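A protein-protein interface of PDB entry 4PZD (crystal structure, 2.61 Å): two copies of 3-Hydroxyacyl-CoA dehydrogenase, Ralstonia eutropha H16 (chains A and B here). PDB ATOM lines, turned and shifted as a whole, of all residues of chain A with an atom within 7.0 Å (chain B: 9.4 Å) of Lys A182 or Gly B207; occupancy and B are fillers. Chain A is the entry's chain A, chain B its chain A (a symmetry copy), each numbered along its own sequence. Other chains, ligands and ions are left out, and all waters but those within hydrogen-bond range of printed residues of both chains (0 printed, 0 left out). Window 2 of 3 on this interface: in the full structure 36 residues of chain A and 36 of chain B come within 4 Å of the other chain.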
ATOM      1  N   LEU A 153     -18.355  17.471 -21.301  1.00  0.00           N
ATOM      2  CA  LEU A 153     -18.907  18.552 -22.078  1.00  0.00           C
ATOM      3  C   LEU A 153     -18.255  19.785 -21.559  1.00  0.00           C
ATOM      4  O   LEU A 153     -18.463  20.132 -20.423  1.00  0.00           O
ATOM      5  CB  LEU A 153     -20.405  18.680 -21.833  1.00  0.00           C
ATOM      6  CG  LEU A 153     -21.302  17.502 -22.225  1.00  0.00           C
ATOM      7  CD1 LEU A 153     -22.761  17.837 -21.903  1.00  0.00           C
ATOM      8  CD2 LEU A 153     -21.119  17.150 -23.695  1.00  0.00           C
ATOM      9  N   ILE A 154     -17.500  20.466 -22.401  1.00  0.00           N
ATOM     10  CA  ILE A 154     -16.654  21.538 -21.960  1.00  0.00           C
ATOM     11  C   ILE A 154     -17.098  22.842 -22.597  1.00  0.00           C
ATOM     12  O   ILE A 154     -17.006  23.021 -23.819  1.00  0.00           O
ATOM     13  CB  ILE A 154     -15.200  21.283 -22.342  1.00  0.00           C
ATOM     14  CG1 ILE A 154     -14.730  19.934 -21.769  1.00  0.00           C
ATOM     15  CG2 ILE A 154     -14.315  22.451 -21.876  1.00  0.00           C
ATOM     16  CD1 ILE A 154     -14.295  18.921 -22.814  1.00  0.00           C
ATOM     17  N   ARG A 155     -17.540  23.773 -21.762  1.00  0.00           N
ATOM     18  CA  ARG A 155     -18.005  25.047 -22.245  1.00  0.00           C
ATOM     19  C   ARG A 155     -16.826  25.938 -22.379  1.00  0.00           C
ATOM     20  O   ARG A 155     -16.053  26.096 -21.453  1.00  0.00           O
ATOM     21  CB  ARG A 155     -18.978  25.661 -21.255  1.00  0.00           C
ATOM     22  CG  ARG A 155     -20.228  24.816 -21.084  1.00  0.00           C
ATOM     23  CD  ARG A 155     -21.252  25.444 -20.141  1.00  0.00           C
ATOM     24  NE  ARG A 155     -21.720  26.768 -20.580  1.00  0.00           N
ATOM     25  CZ  ARG A 155     -22.921  27.263 -20.313  1.00  0.00           C
ATOM     26  NH1 ARG A 155     -23.832  26.557 -19.643  1.00  0.00           N
ATOM     27  NH2 ARG A 155     -23.226  28.465 -20.759  1.00  0.00           N
ATOM     28  N   GLY A 156     -16.662  26.506 -23.554  1.00  0.00           N
ATOM     29  CA  GLY A 156     -15.768  27.626 -23.709  1.00  0.00           C
ATOM     30  C   GLY A 156     -16.434  28.735 -22.926  1.00  0.00           C
ATOM     31  O   GLY A 156     -17.604  28.654 -22.550  1.00  0.00           O
ATOM     32  N   LEU A 157     -15.692  29.796 -22.697  1.00  0.00           N
ATOM     33  CA  LEU A 157     -16.261  31.003 -22.142  1.00  0.00           C
ATOM     34  C   LEU A 157     -17.483  31.441 -22.915  1.00  0.00           C
ATOM     35  O   LEU A 157     -18.318  32.080 -22.362  1.00  0.00           O
ATOM     36  CB  LEU A 157     -15.226  32.129 -22.195  1.00  0.00           C
ATOM     37  CG  LEU A 157     -15.223  33.044 -20.990  1.00  0.00           C
ATOM     38  CD1 LEU A 157     -14.797  32.245 -19.763  1.00  0.00           C
ATOM     39  CD2 LEU A 157     -14.294  34.231 -21.195  1.00  0.00           C
ATOM     40  N   THR A 180     -20.469  18.236 -17.147  1.00  0.00           N
ATOM     41  CA  THR A 180     -20.197  19.639 -17.589  1.00  0.00           C
ATOM     42  C   THR A 180     -18.998  20.289 -16.872  1.00  0.00           C
ATOM     43  O   THR A 180     -18.814  20.168 -15.658  1.00  0.00           O
ATOM     44  CB  THR A 180     -21.472  20.517 -17.581  1.00  0.00           C
ATOM     45  OG1 THR A 180     -22.164  20.335 -18.827  1.00  0.00           O
ATOM     46  CG2 THR A 180     -21.170  22.013 -17.441  1.00  0.00           C
ATOM     47  N   VAL A 181     -18.151  20.947 -17.653  1.00  0.00           N
ATOM     48  CA  VAL A 181     -16.881  21.443 -17.125  1.00  0.00           C
ATOM     49  C   VAL A 181     -16.577  22.761 -17.763  1.00  0.00           C
ATOM     50  O   VAL A 181     -16.691  22.875 -18.986  1.00  0.00           O
ATOM     51  CB  VAL A 181     -15.716  20.498 -17.461  1.00  0.00           C
ATOM     52  CG1 VAL A 181     -14.497  20.874 -16.668  1.00  0.00           C
ATOM     53  CG2 VAL A 181     -16.090  19.065 -17.142  1.00  0.00           C
ATOM     54  N   LYS A 182     -16.190  23.751 -16.964  1.00  0.00           N
ATOM     55  CA  LYS A 182     -15.717  25.010 -17.554  1.00  0.00           C
ATOM     56  C   LYS A 182     -14.353  24.765 -18.160  1.00  0.00           C
ATOM     57  O   LYS A 182     -13.498  24.220 -17.507  1.00  0.00           O
ATOM     58  CB  LYS A 182     -15.580  26.118 -16.516  1.00  0.00           C
ATOM     59  CG  LYS A 182     -16.884  26.498 -15.860  1.00  0.00           C
ATOM     60  CD  LYS A 182     -16.753  27.849 -15.198  1.00  0.00           C
ATOM     61  CE  LYS A 182     -17.920  28.082 -14.234  1.00  0.00           C
ATOM     62  NZ  LYS A 182     -18.020  29.513 -13.802  1.00  0.00           N
ATOM     63  N   ASN A 183     -14.136  25.193 -19.397  1.00  0.00           N
ATOM     64  CA  ASN A 183     -12.815  25.051 -20.012  1.00  0.00           C
ATOM     65  C   ASN A 183     -11.658  25.360 -19.015  1.00  0.00           C
ATOM     66  O   ASN A 183     -11.647  26.419 -18.396  1.00  0.00           O
ATOM     67  CB  ASN A 183     -12.741  25.926 -21.243  1.00  0.00           C
ATOM     68  CG  ASN A 183     -11.498  25.665 -22.055  1.00  0.00           C
ATOM     69  OD1 ASN A 183     -11.224  24.534 -22.442  1.00  0.00           O
ATOM     70  ND2 ASN A 183     -10.726  26.721 -22.318  1.00  0.00           N
ATOM     71  N   SER A 184     -10.733  24.404 -18.842  1.00  0.00           N
ATOM     72  CA  SER A 184      -9.649  24.464 -17.822  1.00  0.00           C
ATOM     73  C   SER A 184      -8.653  23.327 -18.103  1.00  0.00           C
ATOM     74  O   SER A 184      -9.044  22.197 -18.380  1.00  0.00           O
ATOM     75  CB  SER A 184     -10.215  24.283 -16.401  1.00  0.00           C
ATOM     76  OG  SER A 184      -9.222  23.956 -15.403  1.00  0.00           O
ATOM     77  N   PRO A 185      -7.368  23.598 -17.972  1.00  0.00           N
ATOM     78  CA  PRO A 185      -6.447  22.557 -18.346  1.00  0.00           C
ATOM     79  C   PRO A 185      -6.761  21.180 -17.671  1.00  0.00           C
ATOM     80  O   PRO A 185      -6.991  21.115 -16.458  1.00  0.00           O
ATOM     81  CB  PRO A 185      -5.101  23.148 -17.919  1.00  0.00           C
ATOM     82  CG  PRO A 185      -5.292  24.642 -17.985  1.00  0.00           C
ATOM     83  CD  PRO A 185      -6.687  24.799 -17.466  1.00  0.00           C
ATOM     84  N   PHE A 187      -9.456  19.526 -17.991  1.00  0.00           N
ATOM     85  CA  PHE A 187     -10.872  19.509 -17.622  1.00  0.00           C
ATOM     86  C   PHE A 187     -11.145  18.957 -16.205  1.00  0.00           C
ATOM     87  O   PHE A 187     -10.719  19.568 -15.218  1.00  0.00           O
ATOM     88  CB  PHE A 187     -11.641  18.813 -18.731  1.00  0.00           C
ATOM     89  CG  PHE A 187     -11.242  19.298 -20.108  1.00  0.00           C
ATOM     90  CD1 PHE A 187     -11.105  20.650 -20.362  1.00  0.00           C
ATOM     91  CD2 PHE A 187     -10.970  18.396 -21.133  1.00  0.00           C
ATOM     92  CE1 PHE A 187     -10.713  21.096 -21.602  1.00  0.00           C
ATOM     93  CE2 PHE A 187     -10.581  18.844 -22.382  1.00  0.00           C
ATOM     94  CZ  PHE A 187     -10.460  20.199 -22.614  1.00  0.00           C
ATOM     95  N   VAL A 188     -11.837  17.838 -16.085  1.00  0.00           N
ATOM     96  CA  VAL A 188     -12.013  17.231 -14.786  1.00  0.00           C
ATOM     97  C   VAL A 188     -11.206  15.948 -14.706  1.00  0.00           C
ATOM     98  O   VAL A 188     -10.502  15.710 -13.737  1.00  0.00           O
ATOM     99  CB  VAL A 188     -13.531  16.969 -14.505  1.00  0.00           C
ATOM    100  CG1 VAL A 188     -13.750  15.856 -13.489  1.00  0.00           C
ATOM    101  CG2 VAL A 188     -14.239  18.239 -14.034  1.00  0.00           C
ATOM    102  N   ALA B 200      -9.507  17.056  -6.379  1.00  0.00           N
ATOM    103  CA  ALA B 200     -10.975  17.124  -6.553  1.00  0.00           C
ATOM    104  C   ALA B 200     -11.510  18.328  -5.833  1.00  0.00           C
ATOM    105  O   ALA B 200     -12.307  19.063  -6.387  1.00  0.00           O
ATOM    106  CB  ALA B 200     -11.674  15.888  -6.015  1.00  0.00           C
ATOM    107  N   PHE B 201     -11.063  18.558  -4.605  1.00  0.00           N
ATOM    108  CA  PHE B 201     -11.539  19.747  -3.909  1.00  0.00           C
ATOM    109  C   PHE B 201     -11.088  20.991  -4.641  1.00  0.00           C
ATOM    110  O   PHE B 201     -11.846  21.950  -4.714  1.00  0.00           O
ATOM    111  CB  PHE B 201     -11.112  19.803  -2.445  1.00  0.00           C
ATOM    112  CG  PHE B 201     -11.944  18.959  -1.564  1.00  0.00           C
ATOM    113  CD1 PHE B 201     -11.737  17.603  -1.489  1.00  0.00           C
ATOM    114  CD2 PHE B 201     -12.978  19.514  -0.820  1.00  0.00           C
ATOM    115  CE1 PHE B 201     -12.516  16.813  -0.664  1.00  0.00           C
ATOM    116  CE2 PHE B 201     -13.772  18.732   0.007  1.00  0.00           C
ATOM    117  CZ  PHE B 201     -13.532  17.378   0.095  1.00  0.00           C
ATOM    118  N   CYS B 202      -9.861  20.998  -5.154  1.00  0.00           N
ATOM    119  CA  CYS B 202      -9.405  22.147  -5.916  1.00  0.00           C
ATOM    120  C   CYS B 202     -10.345  22.406  -7.121  1.00  0.00           C
ATOM    121  O   CYS B 202     -10.713  23.557  -7.414  1.00  0.00           O
ATOM    122  CB  CYS B 202      -7.919  21.997  -6.325  1.00  0.00           C
ATOM    123  SG  CYS B 202      -6.668  22.249  -5.007  1.00  0.00           S
ATOM    124  N   VAL B 203     -10.781  21.342  -7.792  1.00  0.00           N
ATOM    125  CA  VAL B 203     -11.669  21.474  -8.953  1.00  0.00           C
ATOM    126  C   VAL B 203     -13.037  22.014  -8.526  1.00  0.00           C
ATOM    127  O   VAL B 203     -13.556  22.938  -9.124  1.00  0.00           O
ATOM    128  CB  VAL B 203     -11.799  20.128  -9.706  1.00  0.00           C
ATOM    129  CG1 VAL B 203     -12.890  20.164 -10.723  1.00  0.00           C
ATOM    130  CG2 VAL B 203     -10.515  19.807 -10.442  1.00  0.00           C
ATOM    131  N   LEU B 204     -13.622  21.417  -7.501  1.00  0.00           N
ATOM    132  CA  LEU B 204     -14.879  21.885  -6.922  1.00  0.00           C
ATOM    133  C   LEU B 204     -14.709  23.332  -6.407  1.00  0.00           C
ATOM    134  O   LEU B 204     -15.548  24.207  -6.605  1.00  0.00           O
ATOM    135  CB  LEU B 204     -15.285  20.949  -5.772  1.00  0.00           C
ATOM    136  CG  LEU B 204     -16.555  21.297  -4.954  1.00  0.00           C
ATOM    137  CD1 LEU B 204     -17.768  21.249  -5.844  1.00  0.00           C
ATOM    138  CD2 LEU B 204     -16.770  20.353  -3.778  1.00  0.00           C
ATOM    139  N   GLY B 205     -13.589  23.579  -5.769  1.00  0.00           N
ATOM    140  CA  GLY B 205     -13.293  24.901  -5.235  1.00  0.00           C
ATOM    141  C   GLY B 205     -13.337  25.964  -6.294  1.00  0.00           C
ATOM    142  O   GLY B 205     -13.825  27.026  -6.056  1.00  0.00           O
ATOM    143  N   GLU B 206     -12.862  25.647  -7.493  1.00  0.00           N
ATOM    144  CA  GLU B 206     -12.747  26.640  -8.583  1.00  0.00           C
ATOM    145  C   GLU B 206     -14.017  26.797  -9.394  1.00  0.00           C
ATOM    146  O   GLU B 206     -14.009  27.427 -10.455  1.00  0.00           O
ATOM    147  CB  GLU B 206     -11.616  26.217  -9.549  1.00  0.00           C
ATOM    148  CG  GLU B 206     -10.234  26.218  -8.908  1.00  0.00           C
ATOM    149  CD  GLU B 206      -9.201  25.380  -9.658  1.00  0.00           C
ATOM    150  OE1 GLU B 206      -9.397  25.072 -10.866  1.00  0.00           O
ATOM    151  OE2 GLU B 206      -8.167  25.037  -9.031  1.00  0.00           O
ATOM    152  N   GLY B 207     -15.099  26.169  -8.959  1.00  0.00           N
ATOM    153  CA  GLY B 207     -16.317  26.200  -9.753  1.00  0.00           C
ATOM    154  C   GLY B 207     -16.344  25.464 -11.096  1.00  0.00           C
ATOM    155  O   GLY B 207     -17.212  25.726 -11.906  1.00  0.00           O
ATOM    156  N   LEU B 208     -15.447  24.529 -11.352  1.00  0.00           N
ATOM    157  CA  LEU B 208     -15.356  23.959 -12.707  1.00  0.00           C
ATOM    158  C   LEU B 208     -16.490  23.004 -13.018  1.00  0.00           C
ATOM    159  O   LEU B 208     -16.961  22.935 -14.157  1.00  0.00           O
ATOM    160  CB  LEU B 208     -14.013  23.260 -12.921  1.00  0.00           C
ATOM    161  CG  LEU B 208     -12.801  24.189 -12.710  1.00  0.00           C
ATOM    162  CD1 LEU B 208     -11.522  23.496 -13.090  1.00  0.00           C
ATOM    163  CD2 LEU B 208     -12.923  25.450 -13.524  1.00  0.00           C
ATOM    164  N   ALA B 209     -16.958  22.309 -12.000  1.00  0.00           N
ATOM    165  CA  ALA B 209     -17.970  21.307 -12.172  1.00  0.00           C
ATOM    166  C   ALA B 209     -18.693  21.057 -10.855  1.00  0.00           C
ATOM    167  O   ALA B 209     -18.213  21.420  -9.810  1.00  0.00           O
ATOM    168  CB  ALA B 209     -17.308  20.028 -12.671  1.00  0.00           C
ATOM    169  N   SER B 210     -19.841  20.405 -10.910  1.00  0.00           N
ATOM    170  CA  SER B 210     -20.544  20.028  -9.691  1.00  0.00           C
ATOM    171  C   SER B 210     -19.854  18.820  -9.073  1.00  0.00           C
ATOM    172  O   SER B 210     -19.217  18.033  -9.795  1.00  0.00           O
ATOM    173  CB  SER B 210     -22.015  19.698  -9.972  1.00  0.00           C
ATOM    174  OG  SER B 210     -22.152  18.464 -10.673  1.00  0.00           O
ATOM    175  N   PRO B 211     -19.995  18.659  -7.745  1.00  0.00           N
ATOM    176  CA  PRO B 211     -19.440  17.506  -7.047  1.00  0.00           C
ATOM    177  C   PRO B 211     -19.883  16.189  -7.696  1.00  0.00           C
ATOM    178  O   PRO B 211     -19.037  15.426  -8.177  1.00  0.00           O
ATOM    179  CB  PRO B 211     -20.013  17.620  -5.628  1.00  0.00           C
ATOM    180  CG  PRO B 211     -20.522  19.008  -5.491  1.00  0.00           C
ATOM    181  CD  PRO B 211     -20.786  19.536  -6.864  1.00  0.00           C
ATOM    182  N   GLU B 213     -21.067  15.419 -10.493  1.00  0.00           N
ATOM    183  CA  GLU B 213     -20.412  15.226 -11.796  1.00  0.00           C
ATOM    184  C   GLU B 213     -18.907  14.949 -11.707  1.00  0.00           C
ATOM    185  O   GLU B 213     -18.380  14.234 -12.544  1.00  0.00           O
ATOM    186  CB  GLU B 213     -20.610  16.428 -12.695  1.00  0.00           C
ATOM    187  CG  GLU B 213     -22.003  16.570 -13.277  1.00  0.00           C
ATOM    188  CD  GLU B 213     -22.167  17.863 -14.067  1.00  0.00           C
ATOM    189  OE1 GLU B 213     -21.533  18.898 -13.698  1.00  0.00           O
ATOM    190  OE2 GLU B 213     -22.924  17.842 -15.071  1.00  0.00           O
ATOM    191  N   ILE B 214     -18.227  15.528 -10.717  1.00  0.00           N
ATOM    192  CA  ILE B 214     -16.804  15.282 -10.528  1.00  0.00           C
ATOM    193  C   ILE B 214     -16.677  13.826 -10.169  1.00  0.00           C
ATOM    194  O   ILE B 214     -15.801  13.107 -10.667  1.00  0.00           O
ATOM    195  CB  ILE B 214     -16.227  16.124  -9.369  1.00  0.00           C
ATOM    196  CG1 ILE B 214     -16.066  17.592  -9.762  1.00  0.00           C
ATOM    197  CG2 ILE B 214     -14.898  15.575  -8.875  1.00  0.00           C
ATOM    198  CD1 ILE B 214     -15.438  18.416  -8.661  1.00  0.00           C
ATOM    199  N   LEU B 261     -11.168  25.036  -0.094  1.00  0.00           N
ATOM    200  CA  LEU B 261     -12.512  24.544   0.219  1.00  0.00           C
ATOM    201  C   LEU B 261     -12.479  23.450   1.260  1.00  0.00           C
ATOM    202  O   LEU B 261     -13.417  23.290   2.056  1.00  0.00           O
ATOM    203  CB  LEU B 261     -13.170  23.996  -1.033  1.00  0.00           C
ATOM    204  CG  LEU B 261     -14.667  23.692  -1.000  1.00  0.00           C
ATOM    205  CD1 LEU B 261     -15.504  24.772  -0.300  1.00  0.00           C
ATOM    206  CD2 LEU B 261     -15.165  23.444  -2.435  1.00  0.00           C
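Among the printed residues, merely in contact across the chains: Ser A184 with Leu B208, Val A181 with Leu B208, Thr A180 with Ala B209, Lys A182 with Gly B207, Thr A180 with Leu B208 and Val A188 with Ala B209.
Lys A182 touches just these residues of chain B: Gly B207 and Leu B208. Of the printed residues of chain A, Gly B207 touches Lys A182 (3.4 Å). Of chain B, only Leu B208 (3.3 Å) comes within 4 Å of Val A181. Printed residues of chain B within 4 Å of Ser A184: Leu B208 (3.3 Å). Of the printed residues of chain B, Thr A180 touches Leu B208 (3.7 Å), Ala B209 (3.3 Å) and Glu B213 (3.2 Å). Printed residues of chain B within 4 Å of Val A188: Ala B209. Of the printed residues of chain A, Ala B209 touches Thr A180 and Val A188. Of the printed residues of chain A, Leu B208 touches Thr A180 (3.7 Å), Val A181 (3.3 Å), Lys A182 (3.0 Å) and Ser A184 (3.3 Å). Of the printed residues of chain A, Glu B213 touches Thr A180. The nearest residue of chain B that does not touch Lys A182 is Ala B209 (5.2 Å).
Hydrophobic or aromatic side chains of chain B that line the printed part of chain A: Leu B208 and Ala B209. Of the 13 printed residues of chain A, 5 touch a printed residue of chain B. Hydrophobic or aromatic side chains of chain A within 4 Å of the printed part of chain B: Val A188. Among the printed residues, no Asp or Glu carboxylate lies within 4 Å of a Lys or Arg side-chain nitrogen of the other chain.
No position is printed for both chains. Of the 8 pairs that touch across the chains among the printed residues, none has its exchanged pair printed and touching as well.
O of Leu A153 lies within hydrogen-bond range of N of Val A181, 2.9 Å away. The backbone carbonyl oxygen (O) of Val B203 is in hydrogen-bond range of the backbone NH (N) of Leu B208, at 3.3 Å. The backbone NH of Arg A155 lies within hydrogen-bond range of the backbone carbonyl oxygen of Val A181, at 3.0 Å. The side-chain hydroxyl of Ser B210 sits at hydrogen-bond distance from the side-chain carboxylate of Glu B213 (3.1 Å).
The backbone NH (N) of Lys A182 sits at hydrogen-bond distance from the backbone carbonyl oxygen (O) of Leu B208 (3.0 Å). The backbone NH of Thr A180 is in hydrogen-bond range of the side-chain carboxylate of Glu B213, 3.2 Å away.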
